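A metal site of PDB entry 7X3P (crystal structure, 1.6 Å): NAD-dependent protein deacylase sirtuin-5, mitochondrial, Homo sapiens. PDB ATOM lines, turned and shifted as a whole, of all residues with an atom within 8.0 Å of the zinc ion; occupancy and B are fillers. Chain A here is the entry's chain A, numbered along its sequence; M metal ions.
The backbone NH (N) of Cys 133 sits at hydrogen-bond distance from the backbone carbonyl oxygen (O) of Val 138 (2.9 Å).
The side-chain sulfur (SG) of Cys 133 lies close to the backbone NH (N) of Ser 135 (3.3 Å).
N of Val 138 sits close to SG of Cys 136 (3.6 Å).
The backbone carbonyl oxygen of Gly 181 sits at hydrogen-bond distance from the backbone NH of Cys 174, at 2.7 Å.
N of Glu 176 lies close to SG of Cys 174 (3.5 Å).
The side-chain sulfur (SG) of Cys 179 sits close to the backbone NH (N) of Gly 181 (3.4 Å).
The zinc ion is bound by SG of Cys 179 (2.3 Å).
SG of Cys 174 is bound to the zinc ion (2.3 Å).
The zinc ion is bound by SG of Cys 133, at 2.3 Å.
SG of Cys 136 binds the zinc ion, 2.4 Å away.
The zinc ion has four donor atoms within binding distance.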
ATOM      1  N   ARG A 132      -1.685   2.597 -15.326  1.00  0.00           N
ATOM      2  CA  ARG A 132      -2.337   1.487 -16.016  1.00  0.00           C
ATOM      3  C   ARG A 132      -1.865   0.200 -15.375  1.00  0.00           C
ATOM      4  O   ARG A 132      -0.676  -0.013 -15.174  1.00  0.00           O
ATOM      5  CB  ARG A 132      -2.050   1.496 -17.522  1.00  0.00           C
ATOM      6  CG  ARG A 132      -2.831   0.372 -18.159  1.00  0.00           C
ATOM      7  CD  ARG A 132      -3.025   0.449 -19.612  1.00  0.00           C
ATOM      8  NE  ARG A 132      -1.857   0.074 -20.392  1.00  0.00           N
ATOM      9  CZ  ARG A 132      -0.995   0.941 -20.912  1.00  0.00           C
ATOM     10  NH1 ARG A 132      -1.149   2.207 -20.658  1.00  0.00           N
ATOM     11  NH2 ARG A 132       0.013   0.563 -21.677  1.00  0.00           N
ATOM     12  N   CYS A 133      -2.806  -0.684 -15.051  1.00  0.00           N
ATOM     13  CA  CYS A 133      -2.408  -1.956 -14.481  1.00  0.00           C
ATOM     14  C   CYS A 133      -1.931  -2.935 -15.546  1.00  0.00           C
ATOM     15  O   CYS A 133      -2.615  -3.173 -16.536  1.00  0.00           O
ATOM     16  CB  CYS A 133      -3.582  -2.510 -13.697  1.00  0.00           C
ATOM     17  SG  CYS A 133      -3.179  -4.112 -12.911  1.00  0.00           S
ATOM     18  N   THR A 134      -0.740  -3.484 -15.333  1.00  0.00           N
ATOM     19  CA  THR A 134      -0.167  -4.447 -16.273  1.00  0.00           C
ATOM     20  C   THR A 134      -0.861  -5.792 -16.206  1.00  0.00           C
ATOM     21  O   THR A 134      -0.590  -6.628 -17.070  1.00  0.00           O
ATOM     22  CB  THR A 134       1.330  -4.636 -16.043  1.00  0.00           C
ATOM     23  OG1 THR A 134       1.599  -5.213 -14.760  1.00  0.00           O
ATOM     24  CG2 THR A 134       2.096  -3.294 -16.195  1.00  0.00           C
ATOM     25  N   SER A 135      -1.711  -6.036 -15.209  1.00  0.00           N
ATOM     26  CA  SER A 135      -2.472  -7.279 -15.149  1.00  0.00           C
ATOM     27  C   SER A 135      -3.882  -7.122 -15.711  1.00  0.00           C
ATOM     28  O   SER A 135      -4.280  -7.886 -16.601  1.00  0.00           O
ATOM     29  CB  SER A 135      -2.555  -7.780 -13.701  1.00  0.00           C
ATOM     30  OG  SER A 135      -1.302  -8.238 -13.223  1.00  0.00           O
ATOM     31  N   CYS A 136      -4.659  -6.164 -15.214  1.00  0.00           N
ATOM     32  CA  CYS A 136      -6.056  -6.054 -15.596  1.00  0.00           C
ATOM     33  C   CYS A 136      -6.343  -4.936 -16.582  1.00  0.00           C
ATOM     34  O   CYS A 136      -7.468  -4.861 -17.081  1.00  0.00           O
ATOM     35  CB  CYS A 136      -6.938  -5.855 -14.346  1.00  0.00           C
ATOM     36  SG  CYS A 136      -6.849  -4.201 -13.589  1.00  0.00           S
ATOM     37  N   GLY A 137      -5.362  -4.077 -16.870  1.00  0.00           N
ATOM     38  CA  GLY A 137      -5.513  -3.023 -17.853  1.00  0.00           C
ATOM     39  C   GLY A 137      -6.248  -1.776 -17.403  1.00  0.00           C
ATOM     40  O   GLY A 137      -6.375  -0.839 -18.216  1.00  0.00           O
ATOM     41  N   VAL A 138      -6.730  -1.717 -16.168  1.00  0.00           N
ATOM     42  CA  VAL A 138      -7.487  -0.548 -15.716  1.00  0.00           C
ATOM     43  C   VAL A 138      -6.586   0.677 -15.682  1.00  0.00           C
ATOM     44  O   VAL A 138      -5.441   0.628 -15.209  1.00  0.00           O
ATOM     45  CB  VAL A 138      -8.121  -0.810 -14.344  1.00  0.00           C
ATOM     46  CG1 VAL A 138      -8.737   0.457 -13.731  1.00  0.00           C
ATOM     47  CG2 VAL A 138      -9.205  -1.855 -14.506  1.00  0.00           C
ATOM     48  N   VAL A 139      -7.142   1.780 -16.171  1.00  0.00           N
ATOM     49  CA  VAL A 139      -6.504   3.098 -16.154  1.00  0.00           C
ATOM     50  C   VAL A 139      -7.155   3.926 -15.060  1.00  0.00           C
ATOM     51  O   VAL A 139      -8.390   4.004 -14.978  1.00  0.00           O
ATOM     52  CB  VAL A 139      -6.645   3.782 -17.517  1.00  0.00           C
ATOM     53  CG1 VAL A 139      -6.048   5.189 -17.494  1.00  0.00           C
ATOM     54  CG2 VAL A 139      -6.013   2.956 -18.616  1.00  0.00           C
ATOM     55  N   ARG A 173       0.917  -0.629  -6.898  1.00  0.00           N
ATOM     56  CA  ARG A 173       0.105  -1.795  -7.180  1.00  0.00           C
ATOM     57  C   ARG A 173      -1.349  -1.406  -7.383  1.00  0.00           C
ATOM     58  O   ARG A 173      -1.854  -0.438  -6.804  1.00  0.00           O
ATOM     59  CB  ARG A 173       0.168  -2.832  -6.038  1.00  0.00           C
ATOM     60  CG  ARG A 173       1.562  -3.250  -5.604  1.00  0.00           C
ATOM     61  CD  ARG A 173       2.419  -3.838  -6.724  1.00  0.00           C
ATOM     62  NE  ARG A 173       1.882  -5.095  -7.246  1.00  0.00           N
ATOM     63  CZ  ARG A 173       2.593  -6.054  -7.813  1.00  0.00           C
ATOM     64  NH1 ARG A 173       3.903  -5.942  -7.965  1.00  0.00           N
ATOM     65  NH2 ARG A 173       1.984  -7.143  -8.241  1.00  0.00           N
ATOM     66  N   CYS A 174      -2.029  -2.230  -8.175  1.00  0.00           N
ATOM     67  CA  CYS A 174      -3.423  -2.020  -8.515  1.00  0.00           C
ATOM     68  C   CYS A 174      -4.305  -2.151  -7.282  1.00  0.00           C
ATOM     69  O   CYS A 174      -4.180  -3.106  -6.518  1.00  0.00           O
ATOM     70  CB  CYS A 174      -3.855  -3.034  -9.580  1.00  0.00           C
ATOM     71  SG  CYS A 174      -5.464  -2.793 -10.255  1.00  0.00           S
ATOM     72  N   GLU A 175      -5.230  -1.204  -7.118  1.00  0.00           N
ATOM     73  CA  GLU A 175      -6.144  -1.216  -5.984  1.00  0.00           C
ATOM     74  C   GLU A 175      -7.529  -1.727  -6.351  1.00  0.00           C
ATOM     75  O   GLU A 175      -8.445  -1.684  -5.513  1.00  0.00           O
ATOM     76  CB  GLU A 175      -6.231   0.181  -5.382  1.00  0.00           C
ATOM     77  CG  GLU A 175      -4.895   0.664  -4.833  1.00  0.00           C
ATOM     78  CD  GLU A 175      -4.977   2.093  -4.313  1.00  0.00           C
ATOM     79  OE1 GLU A 175      -5.457   2.261  -3.191  1.00  0.00           O
ATOM     80  OE2 GLU A 175      -4.573   3.037  -5.040  1.00  0.00           O
ATOM     81  N   GLU A 176      -7.717  -2.237  -7.569  1.00  0.00           N
ATOM     82  CA  GLU A 176      -8.979  -2.865  -7.910  1.00  0.00           C
ATOM     83  C   GLU A 176      -9.144  -4.091  -7.052  1.00  0.00           C
ATOM     84  O   GLU A 176      -8.184  -4.841  -6.820  1.00  0.00           O
ATOM     85  CB  GLU A 176      -9.024  -3.259  -9.395  1.00  0.00           C
ATOM     86  CG  GLU A 176      -8.940  -2.074 -10.373  1.00  0.00           C
ATOM     87  CD  GLU A 176     -10.117  -1.159 -10.261  1.00  0.00           C
ATOM     88  OE1 GLU A 176     -11.238  -1.612 -10.568  1.00  0.00           O
ATOM     89  OE2 GLU A 176      -9.912  -0.004  -9.841  1.00  0.00           O
ATOM     90  N   ALA A 177     -10.370  -4.325  -6.595  1.00  0.00           N
ATOM     91  CA  ALA A 177     -10.616  -5.482  -5.746  1.00  0.00           C
ATOM     92  C   ALA A 177     -10.233  -6.770  -6.477  1.00  0.00           C
ATOM     93  O   ALA A 177     -10.671  -7.026  -7.590  1.00  0.00           O
ATOM     94  CB  ALA A 177     -12.088  -5.514  -5.355  1.00  0.00           C
ATOM     95  N   GLY A 178      -9.377  -7.560  -5.842  1.00  0.00           N
ATOM     96  CA  GLY A 178      -9.018  -8.846  -6.393  1.00  0.00           C
ATOM     97  C   GLY A 178      -7.959  -8.815  -7.470  1.00  0.00           C
ATOM     98  O   GLY A 178      -7.701  -9.852  -8.100  1.00  0.00           O
ATOM     99  N   CYS A 179      -7.314  -7.682  -7.716  1.00  0.00           N
ATOM    100  CA  CYS A 179      -6.250  -7.684  -8.708  1.00  0.00           C
ATOM    101  C   CYS A 179      -4.874  -7.624  -8.056  1.00  0.00           C
ATOM    102  O   CYS A 179      -4.209  -8.660  -7.927  1.00  0.00           O
ATOM    103  CB  CYS A 179      -6.455  -6.521  -9.664  1.00  0.00           C
ATOM    104  SG  CYS A 179      -5.149  -6.504 -10.951  1.00  0.00           S
ATOM    105  N   GLY A 180      -4.421  -6.430  -7.650  1.00  0.00           N
ATOM    106  CA  GLY A 180      -3.123  -6.281  -7.010  1.00  0.00           C
ATOM    107  C   GLY A 180      -1.925  -6.276  -7.949  1.00  0.00           C
ATOM    108  O   GLY A 180      -0.789  -6.403  -7.486  1.00  0.00           O
ATOM    109  N   GLY A 181      -2.179  -6.186  -9.237  1.00  0.00           N
ATOM    110  CA  GLY A 181      -1.102  -6.220 -10.216  1.00  0.00           C
ATOM    111  C   GLY A 181      -0.166  -5.031 -10.128  1.00  0.00           C
ATOM    112  O   GLY A 181      -0.402  -4.024  -9.438  1.00  0.00           O
ATOM    113  N   LEU A 182       0.929  -5.150 -10.850  1.00  0.00           N
ATOM    114  CA  LEU A 182       1.921  -4.075 -10.931  1.00  0.00           C
ATOM    115  C   LEU A 182       1.419  -2.973 -11.852  1.00  0.00           C
ATOM    116  O   LEU A 182       1.050  -3.236 -12.999  1.00  0.00           O
ATOM    117  CB  LEU A 182       3.255  -4.591 -11.455  1.00  0.00           C
ATOM    118  CG  LEU A 182       4.345  -3.574 -11.714  1.00  0.00           C
ATOM    119  CD1 LEU A 182       4.823  -2.892 -10.474  1.00  0.00           C
ATOM    120  CD2 LEU A 182       5.502  -4.268 -12.422  1.00  0.00           C
ATOM    121  N   LEU A 183       1.451  -1.731 -11.359  1.00  0.00           N
ATOM    122  CA  LEU A 183       1.089  -0.594 -12.198  1.00  0.00           C
ATOM    123  C   LEU A 183       2.295  -0.128 -12.990  1.00  0.00           C
ATOM    124  O   LEU A 183       3.440  -0.216 -12.539  1.00  0.00           O
ATOM    125  CB  LEU A 183       0.577   0.558 -11.355  1.00  0.00           C
ATOM    126  CG  LEU A 183      -0.627   0.262 -10.472  1.00  0.00           C
ATOM    127  CD1 LEU A 183      -1.020   1.516  -9.719  1.00  0.00           C
ATOM    128  CD2 LEU A 183      -1.771  -0.283 -11.331  1.00  0.00           C
HETATM  129 ZN    ZN M   1      -5.245  -4.430 -11.871  1.00  0.00          ZN
